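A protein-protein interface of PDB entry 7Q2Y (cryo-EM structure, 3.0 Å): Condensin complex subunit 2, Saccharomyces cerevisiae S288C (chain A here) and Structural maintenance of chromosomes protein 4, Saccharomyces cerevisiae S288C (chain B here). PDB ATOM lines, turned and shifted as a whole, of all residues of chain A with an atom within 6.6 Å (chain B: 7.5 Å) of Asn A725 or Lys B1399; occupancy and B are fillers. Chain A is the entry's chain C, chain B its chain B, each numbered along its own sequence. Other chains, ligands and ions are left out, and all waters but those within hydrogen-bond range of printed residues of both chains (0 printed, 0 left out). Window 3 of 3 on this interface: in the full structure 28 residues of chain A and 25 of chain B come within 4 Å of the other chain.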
ATOM      1  N   LEU A 720      -4.803  15.240 -11.319  1.00  0.00           N
ATOM      2  CA  LEU A 720      -4.004  16.052 -10.408  1.00  0.00           C
ATOM      3  C   LEU A 720      -4.861  17.101  -9.713  1.00  0.00           C
ATOM      4  O   LEU A 720      -4.679  17.375  -8.521  1.00  0.00           O
ATOM      5  CB  LEU A 720      -2.852  16.710 -11.167  1.00  0.00           C
ATOM      6  CG  LEU A 720      -1.764  17.377 -10.325  1.00  0.00           C
ATOM      7  CD1 LEU A 720      -0.783  16.339  -9.802  1.00  0.00           C
ATOM      8  CD2 LEU A 720      -1.040  18.440 -11.134  1.00  0.00           C
ATOM      9  N   LEU A 721      -5.802  17.705 -10.444  1.00  0.00           N
ATOM     10  CA  LEU A 721      -6.718  18.659  -9.830  1.00  0.00           C
ATOM     11  C   LEU A 721      -7.585  17.989  -8.772  1.00  0.00           C
ATOM     12  O   LEU A 721      -7.822  18.557  -7.700  1.00  0.00           O
ATOM     13  CB  LEU A 721      -7.591  19.312 -10.901  1.00  0.00           C
ATOM     14  CG  LEU A 721      -6.887  20.275 -11.858  1.00  0.00           C
ATOM     15  CD1 LEU A 721      -7.659  20.379 -13.162  1.00  0.00           C
ATOM     16  CD2 LEU A 721      -6.717  21.641 -11.217  1.00  0.00           C
ATOM     17  N   HIS A 722      -8.069  16.777  -9.057  1.00  0.00           N
ATOM     18  CA  HIS A 722      -8.860  16.045  -8.073  1.00  0.00           C
ATOM     19  C   HIS A 722      -8.035  15.723  -6.832  1.00  0.00           C
ATOM     20  O   HIS A 722      -8.525  15.837  -5.701  1.00  0.00           O
ATOM     21  CB  HIS A 722      -9.416  14.763  -8.693  1.00  0.00           C
ATOM     22  CG  HIS A 722     -10.724  14.949  -9.396  1.00  0.00           C
ATOM     23  ND1 HIS A 722     -10.817  15.146 -10.757  1.00  0.00           N
ATOM     24  CD2 HIS A 722     -11.995  14.964  -8.926  1.00  0.00           C
ATOM     25  CE1 HIS A 722     -12.087  15.276 -11.095  1.00  0.00           C
ATOM     26  NE2 HIS A 722     -12.822  15.170 -10.003  1.00  0.00           N
ATOM     27  N   LEU A 723      -6.780  15.312  -7.024  1.00  0.00           N
ATOM     28  CA  LEU A 723      -5.911  15.024  -5.886  1.00  0.00           C
ATOM     29  C   LEU A 723      -5.649  16.277  -5.061  1.00  0.00           C
ATOM     30  O   LEU A 723      -5.637  16.225  -3.825  1.00  0.00           O
ATOM     31  CB  LEU A 723      -4.597  14.412  -6.369  1.00  0.00           C
ATOM     32  CG  LEU A 723      -4.676  12.960  -6.844  1.00  0.00           C
ATOM     33  CD1 LEU A 723      -3.376  12.546  -7.508  1.00  0.00           C
ATOM     34  CD2 LEU A 723      -5.011  12.034  -5.686  1.00  0.00           C
ATOM     35  N   ALA A 724      -5.430  17.414  -5.726  1.00  0.00           N
ATOM     36  CA  ALA A 724      -5.254  18.671  -5.006  1.00  0.00           C
ATOM     37  C   ALA A 724      -6.519  19.049  -4.247  1.00  0.00           C
ATOM     38  O   ALA A 724      -6.450  19.621  -3.154  1.00  0.00           O
ATOM     39  CB  ALA A 724      -4.855  19.782  -5.975  1.00  0.00           C
ATOM     40  N   ASN A 725      -7.685  18.749  -4.822  1.00  0.00           N
ATOM     41  CA  ASN A 725      -8.941  18.964  -4.111  1.00  0.00           C
ATOM     42  C   ASN A 725      -9.016  18.095  -2.863  1.00  0.00           C
ATOM     43  O   ASN A 725      -9.470  18.547  -1.806  1.00  0.00           O
ATOM     44  CB  ASN A 725     -10.118  18.680  -5.046  1.00  0.00           C
ATOM     45  CG  ASN A 725     -11.449  19.135  -4.474  1.00  0.00           C
ATOM     46  OD1 ASN A 725     -11.521  19.655  -3.362  1.00  0.00           O
ATOM     47  ND2 ASN A 725     -12.516  18.941  -5.241  1.00  0.00           N
ATOM     48  N   GLU A 726      -8.566  16.842  -2.964  1.00  0.00           N
ATOM     49  CA  GLU A 726      -8.615  15.940  -1.818  1.00  0.00           C
ATOM     50  C   GLU A 726      -7.426  16.152  -0.885  1.00  0.00           C
ATOM     51  O   GLU A 726      -7.605  16.395   0.314  1.00  0.00           O
ATOM     52  CB  GLU A 726      -8.669  14.488  -2.295  1.00  0.00           C
ATOM     53  CG  GLU A 726     -10.071  13.908  -2.360  1.00  0.00           C
ATOM     54  CD  GLU A 726     -10.085  12.465  -2.825  1.00  0.00           C
ATOM     55  OE1 GLU A 726      -9.266  12.115  -3.700  1.00  0.00           O
ATOM     56  OE2 GLU A 726     -10.914  11.683  -2.315  1.00  0.00           O
ATOM     57  N   HIS A 727      -6.210  16.065  -1.415  1.00  0.00           N
ATOM     58  CA  HIS A 727      -5.002  16.180  -0.611  1.00  0.00           C
ATOM     59  C   HIS A 727      -4.579  17.646  -0.513  1.00  0.00           C
ATOM     60  O   HIS A 727      -5.332  18.558  -0.861  1.00  0.00           O
ATOM     61  CB  HIS A 727      -3.897  15.302  -1.193  1.00  0.00           C
ATOM     62  CG  HIS A 727      -4.269  13.856  -1.299  1.00  0.00           C
ATOM     63  ND1 HIS A 727      -4.354  13.027  -0.201  1.00  0.00           N
ATOM     64  CD2 HIS A 727      -4.580  13.091  -2.372  1.00  0.00           C
ATOM     65  CE1 HIS A 727      -4.701  11.815  -0.593  1.00  0.00           C
ATOM     66  NE2 HIS A 727      -4.843  11.826  -1.906  1.00  0.00           N
ATOM     67  N   GLY A 728      -3.364  17.885  -0.027  1.00  0.00           N
ATOM     68  CA  GLY A 728      -2.877  19.238   0.158  1.00  0.00           C
ATOM     69  C   GLY A 728      -1.803  19.650  -0.828  1.00  0.00           C
ATOM     70  O   GLY A 728      -0.842  20.331  -0.457  1.00  0.00           O
ATOM     71  N   LEU A 729      -1.952  19.244  -2.086  1.00  0.00           N
ATOM     72  CA  LEU A 729      -0.991  19.605  -3.117  1.00  0.00           C
ATOM     73  C   LEU A 729      -1.286  20.998  -3.660  1.00  0.00           C
ATOM     74  O   LEU A 729      -2.447  21.390  -3.808  1.00  0.00           O
ATOM     75  CB  LEU A 729      -1.022  18.587  -4.257  1.00  0.00           C
ATOM     76  CG  LEU A 729      -0.800  17.122  -3.880  1.00  0.00           C
ATOM     77  CD1 LEU A 729      -0.944  16.229  -5.102  1.00  0.00           C
ATOM     78  CD2 LEU A 729       0.564  16.937  -3.234  1.00  0.00           C
ATOM     79  N   SER B 166     -15.834  31.856  -4.385  1.00  0.00           N
ATOM     80  CA  SER B 166     -14.957  30.861  -3.778  1.00  0.00           C
ATOM     81  C   SER B 166     -13.507  31.325  -3.737  1.00  0.00           C
ATOM     82  O   SER B 166     -12.759  30.930  -2.836  1.00  0.00           O
ATOM     83  CB  SER B 166     -15.069  29.537  -4.530  1.00  0.00           C
ATOM     84  OG  SER B 166     -14.665  29.681  -5.880  1.00  0.00           O
ATOM     85  N   TYR B 167     -13.092  32.150  -4.696  1.00  0.00           N
ATOM     86  CA  TYR B 167     -11.708  32.605  -4.738  1.00  0.00           C
ATOM     87  C   TYR B 167     -11.401  33.509  -3.549  1.00  0.00           C
ATOM     88  O   TYR B 167     -12.191  34.387  -3.192  1.00  0.00           O
ATOM     89  CB  TYR B 167     -11.433  33.342  -6.048  1.00  0.00           C
ATOM     90  CG  TYR B 167     -11.495  32.456  -7.273  1.00  0.00           C
ATOM     91  CD1 TYR B 167     -12.708  32.157  -7.877  1.00  0.00           C
ATOM     92  CD2 TYR B 167     -10.339  31.916  -7.820  1.00  0.00           C
ATOM     93  CE1 TYR B 167     -12.769  31.347  -8.993  1.00  0.00           C
ATOM     94  CE2 TYR B 167     -10.391  31.105  -8.937  1.00  0.00           C
ATOM     95  CZ  TYR B 167     -11.607  30.824  -9.519  1.00  0.00           C
ATOM     96  OH  TYR B 167     -11.664  30.016 -10.631  1.00  0.00           O
ATOM     97  N   GLY B 185     -12.406  20.967 -14.150  1.00  0.00           N
ATOM     98  CA  GLY B 185     -12.168  20.838 -12.735  1.00  0.00           C
ATOM     99  C   GLY B 185     -13.223  19.997 -12.045  1.00  0.00           C
ATOM    100  O   GLY B 185     -14.252  19.647 -12.630  1.00  0.00           O
ATOM    101  N   PRO B 186     -12.981  19.652 -10.784  1.00  0.00           N
ATOM    102  CA  PRO B 186     -13.970  18.880 -10.025  1.00  0.00           C
ATOM    103  C   PRO B 186     -15.232  19.690  -9.769  1.00  0.00           C
ATOM    104  O   PRO B 186     -15.227  20.922  -9.760  1.00  0.00           O
ATOM    105  CB  PRO B 186     -13.245  18.558  -8.712  1.00  0.00           C
ATOM    106  CG  PRO B 186     -11.789  18.752  -9.017  1.00  0.00           C
ATOM    107  CD  PRO B 186     -11.743  19.862 -10.016  1.00  0.00           C
ATOM    108  N   ASN B 187     -16.333  18.966  -9.572  1.00  0.00           N
ATOM    109  CA  ASN B 187     -17.602  19.610  -9.261  1.00  0.00           C
ATOM    110  C   ASN B 187     -17.506  20.356  -7.937  1.00  0.00           C
ATOM    111  O   ASN B 187     -17.015  19.818  -6.940  1.00  0.00           O
ATOM    112  CB  ASN B 187     -18.723  18.573  -9.208  1.00  0.00           C
ATOM    113  CG  ASN B 187     -19.089  18.040 -10.577  1.00  0.00           C
ATOM    114  OD1 ASN B 187     -18.986  16.842 -10.838  1.00  0.00           O
ATOM    115  ND2 ASN B 187     -19.520  18.930 -11.463  1.00  0.00           N
ATOM    116  N   GLY B 188     -17.980  21.600  -7.930  1.00  0.00           N
ATOM    117  CA  GLY B 188     -17.918  22.436  -6.752  1.00  0.00           C
ATOM    118  C   GLY B 188     -16.611  23.168  -6.550  1.00  0.00           C
ATOM    119  O   GLY B 188     -16.497  23.942  -5.591  1.00  0.00           O
ATOM    120  N   SER B 189     -15.620  22.948  -7.418  1.00  0.00           N
ATOM    121  CA  SER B 189     -14.340  23.634  -7.273  1.00  0.00           C
ATOM    122  C   SER B 189     -14.488  25.136  -7.483  1.00  0.00           C
ATOM    123  O   SER B 189     -13.852  25.932  -6.784  1.00  0.00           O
ATOM    124  CB  SER B 189     -13.319  23.053  -8.250  1.00  0.00           C
ATOM    125  OG  SER B 189     -13.817  23.066  -9.575  1.00  0.00           O
ATOM    126  N   GLY B 190     -15.322  25.541  -8.438  1.00  0.00           N
ATOM    127  CA  GLY B 190     -15.512  26.950  -8.715  1.00  0.00           C
ATOM    128  C   GLY B 190     -15.128  27.347 -10.126  1.00  0.00           C
ATOM    129  O   GLY B 190     -14.699  28.480 -10.361  1.00  0.00           O
ATOM    130  N   ASN B 193     -17.276  29.979 -11.439  1.00  0.00           N
ATOM    131  CA  ASN B 193     -17.091  31.269 -10.786  1.00  0.00           C
ATOM    132  C   ASN B 193     -16.416  32.274 -11.708  1.00  0.00           C
ATOM    133  O   ASN B 193     -16.640  33.479 -11.568  1.00  0.00           O
ATOM    134  CB  ASN B 193     -16.287  31.096  -9.498  1.00  0.00           C
ATOM    135  CG  ASN B 193     -17.124  30.547  -8.360  1.00  0.00           C
ATOM    136  OD1 ASN B 193     -16.598  29.957  -7.416  1.00  0.00           O
ATOM    137  ND2 ASN B 193     -18.435  30.734  -8.446  1.00  0.00           N
ATOM    138  N   VAL B1397      -9.147  24.359 -12.024  1.00  0.00           N
ATOM    139  CA  VAL B1397      -9.369  24.975 -10.723  1.00  0.00           C
ATOM    140  C   VAL B1397      -9.501  23.881  -9.672  1.00  0.00           C
ATOM    141  O   VAL B1397     -10.165  22.863  -9.898  1.00  0.00           O
ATOM    142  CB  VAL B1397     -10.615  25.886 -10.727  1.00  0.00           C
ATOM    143  CG1 VAL B1397     -10.367  27.113 -11.588  1.00  0.00           C
ATOM    144  CG2 VAL B1397     -11.830  25.129 -11.226  1.00  0.00           C
ATOM    145  N   TYR B1398      -8.846  24.085  -8.531  1.00  0.00           N
ATOM    146  CA  TYR B1398      -8.932  23.166  -7.405  1.00  0.00           C
ATOM    147  C   TYR B1398      -9.243  23.950  -6.139  1.00  0.00           C
ATOM    148  O   TYR B1398      -8.684  25.027  -5.912  1.00  0.00           O
ATOM    149  CB  TYR B1398      -7.636  22.357  -7.228  1.00  0.00           C
ATOM    150  CG  TYR B1398      -6.375  23.187  -7.124  1.00  0.00           C
ATOM    151  CD1 TYR B1398      -5.740  23.669  -8.260  1.00  0.00           C
ATOM    152  CD2 TYR B1398      -5.813  23.476  -5.888  1.00  0.00           C
ATOM    153  CE1 TYR B1398      -4.586  24.423  -8.169  1.00  0.00           C
ATOM    154  CE2 TYR B1398      -4.660  24.228  -5.786  1.00  0.00           C
ATOM    155  CZ  TYR B1398      -4.050  24.698  -6.929  1.00  0.00           C
ATOM    156  OH  TYR B1398      -2.900  25.449  -6.832  1.00  0.00           O
ATOM    157  N   LYS B1399     -10.137  23.404  -5.320  1.00  0.00           N
ATOM    158  CA  LYS B1399     -10.631  24.081  -4.129  1.00  0.00           C
ATOM    159  C   LYS B1399     -10.198  23.331  -2.877  1.00  0.00           C
ATOM    160  O   LYS B1399     -10.457  22.130  -2.744  1.00  0.00           O
ATOM    161  CB  LYS B1399     -12.157  24.201  -4.169  1.00  0.00           C
ATOM    162  CG  LYS B1399     -12.749  24.965  -2.998  1.00  0.00           C
ATOM    163  CD  LYS B1399     -14.261  25.065  -3.112  1.00  0.00           C
ATOM    164  CE  LYS B1399     -14.932  23.768  -2.696  1.00  0.00           C
ATOM    165  NZ  LYS B1399     -16.416  23.866  -2.764  1.00  0.00           N
ATOM    166  N   ARG B1400      -9.541  24.044  -1.966  1.00  0.00           N
ATOM    167  CA  ARG B1400      -9.197  23.533  -0.646  1.00  0.00           C
ATOM    168  C   ARG B1400      -9.684  24.521   0.400  1.00  0.00           C
ATOM    169  O   ARG B1400      -9.412  25.723   0.296  1.00  0.00           O
ATOM    170  CB  ARG B1400      -7.687  23.318  -0.501  1.00  0.00           C
ATOM    171  CG  ARG B1400      -7.096  22.324  -1.479  1.00  0.00           C
ATOM    172  CD  ARG B1400      -5.674  21.958  -1.086  1.00  0.00           C
ATOM    173  NE  ARG B1400      -5.640  21.101   0.093  1.00  0.00           N
ATOM    174  CZ  ARG B1400      -5.319  21.514   1.311  1.00  0.00           C
ATOM    175  NH1 ARG B1400      -4.993  22.774   1.550  1.00  0.00           N
ATOM    176  NH2 ARG B1400      -5.322  20.641   2.314  1.00  0.00           N
ATOM    177  N   ASP B1401     -10.398  24.012   1.405  1.00  0.00           N
ATOM    178  CA  ASP B1401     -10.918  24.822   2.507  1.00  0.00           C
ATOM    179  C   ASP B1401     -11.716  26.009   1.964  1.00  0.00           C
ATOM    180  O   ASP B1401     -11.549  27.156   2.384  1.00  0.00           O
ATOM    181  CB  ASP B1401      -9.782  25.277   3.429  1.00  0.00           C
ATOM    182  CG  ASP B1401     -10.279  25.937   4.710  1.00  0.00           C
ATOM    183  OD1 ASP B1401     -11.507  26.077   4.889  1.00  0.00           O
ATOM    184  OD2 ASP B1401      -9.430  26.318   5.543  1.00  0.00           O
ATOM    185  N   ASN B1402     -12.574  25.717   0.983  1.00  0.00           N
ATOM    186  CA  ASN B1402     -13.435  26.715   0.346  1.00  0.00           C
ATOM    187  C   ASN B1402     -12.630  27.849  -0.287  1.00  0.00           C
ATOM    188  O   ASN B1402     -13.095  28.989  -0.359  1.00  0.00           O
ATOM    189  CB  ASN B1402     -14.462  27.278   1.334  1.00  0.00           C
ATOM    190  CG  ASN B1402     -15.346  26.200   1.930  1.00  0.00           C
ATOM    191  OD1 ASN B1402     -15.320  25.956   3.136  1.00  0.00           O
ATOM    192  ND2 ASN B1402     -16.135  25.549   1.084  1.00  0.00           N
ATOM    193  N   ARG B1403     -11.418  27.547  -0.752  1.00  0.00           N
ATOM    194  CA  ARG B1403     -10.571  28.518  -1.434  1.00  0.00           C
ATOM    195  C   ARG B1403     -10.104  27.904  -2.744  1.00  0.00           C
ATOM    196  O   ARG B1403      -9.534  26.810  -2.747  1.00  0.00           O
ATOM    197  CB  ARG B1403      -9.377  28.917  -0.564  1.00  0.00           C
ATOM    198  CG  ARG B1403      -9.759  29.687   0.690  1.00  0.00           C
ATOM    199  CD  ARG B1403      -8.539  30.035   1.525  1.00  0.00           C
ATOM    200  NE  ARG B1403      -7.914  28.850   2.101  1.00  0.00           N
ATOM    201  CZ  ARG B1403      -6.762  28.855   2.758  1.00  0.00           C
ATOM    202  NH1 ARG B1403      -6.077  29.971   2.942  1.00  0.00           N
ATOM    203  NH2 ARG B1403      -6.286  27.711   3.242  1.00  0.00           N
ATOM    204  N   THR B1404     -10.337  28.606  -3.849  1.00  0.00           N
ATOM    205  CA  THR B1404     -10.084  28.073  -5.180  1.00  0.00           C
ATOM    206  C   THR B1404      -8.816  28.671  -5.775  1.00  0.00           C
ATOM    207  O   THR B1404      -8.597  29.885  -5.710  1.00  0.00           O
ATOM    208  CB  THR B1404     -11.269  28.348  -6.109  1.00  0.00           C
ATOM    209  OG1 THR B1404     -12.478  27.893  -5.490  1.00  0.00           O
ATOM    210  CG2 THR B1404     -11.087  27.629  -7.436  1.00  0.00           C
ATOM    211  N   LYS B1405      -7.983  27.809  -6.354  1.00  0.00           N
ATOM    212  CA  LYS B1405      -6.779  28.219  -7.060  1.00  0.00           C
ATOM    213  C   LYS B1405      -6.808  27.644  -8.470  1.00  0.00           C
ATOM    214  O   LYS B1405      -7.218  26.497  -8.673  1.00  0.00           O
ATOM    215  CB  LYS B1405      -5.514  27.759  -6.327  1.00  0.00           C
ATOM    216  CG  LYS B1405      -5.432  28.224  -4.883  1.00  0.00           C
ATOM    217  CD  LYS B1405      -3.990  28.351  -4.424  1.00  0.00           C
ATOM    218  CE  LYS B1405      -3.828  27.898  -2.982  1.00  0.00           C
ATOM    219  NZ  LYS B1405      -4.466  28.847  -2.028  1.00  0.00           N
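The backbone carbonyl oxygen (O) of Lys B1399 lies close to the side-chain amide oxygen (OD1) of Asn A725. The backbone carbonyl oxygen of His A727 lies within hydrogen-bond range of the guanidinium group of Arg B1400, 2.7 Å away.
The backbone carbonyl oxygen of Pro B186 is in hydrogen-bond range of the side-chain hydroxyl of Ser B189, 2.6 Å away. NZ of Lys B1399 is in hydrogen-bond range of O of Gly B188, at 2.8 Å. The backbone carbonyl oxygen (O) of Tyr B1398 lies within hydrogen-bond range of the backbone NH (N) of Lys B1405 (2.9 Å).
Leu A721 touches Val B1397 (CD2 to N, 3.7 Å). Leu A721 touches Tyr B1398 (CD2 to CD1, 3.7 Å). Pro B186 touches His A722. Ala A724 touches Tyr B1398 (CB to CD2, 3.8 Å). O of Ala A724 touches CD of Arg B1400, at 3.2 Å. ND2 of Asn A725 touches CB of Pro B186, 3.6 Å away. Gly A728 touches Arg B1400 (CA to NE, 3.3 Å).
Of chain B, only Tyr B1398 (3.8 Å) and Arg B1400 (3.2 Å) come within 4 Å of Ala A724. Of chain B, only Pro B186 (3.6 Å) and Lys B1399 (2.8 Å) come within 4 Å of Asn A725. Asn B193 touches none of the printed residues of chain A. Printed residues of chain A within 4 Å of Tyr B1398: Leu A721 (3.7 Å) and Ala A724 (3.8 Å). Of chain A, only Asn A725 comes within 4 Å of Lys B1399. Of the printed residues of chain A, Arg B1400 touches Ala A724 (3.2 Å), His A727 (2.7 Å) and Gly A728 (3.3 Å). The nearest residue of chain B that does not touch Asn A725 is Tyr B1398 (4.3 Å).
Printed residues of chain A that touch a printed residue of chain B: Leu A721, His A722, Ala A724, Asn A725, His A727 and Gly A728. Hydrophobic or aromatic side chains of chain A within 4 Å of the printed part of chain B: Leu A721, His A722 and Ala A724. Of the 18 printed residues of chain B, 5 touch a printed residue of chain A. Printed residues of chain B that touch a printed residue of chain A: Pro B186, Val B1397, Tyr B1398, Lys B1399 and Arg B1400. Hydrophobic or aromatic side chains of chain B within 4 Å of the printed part of chain A: Pro B186 and Tyr B1398. Among the printed residues, 9 pairs touch across the chains.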
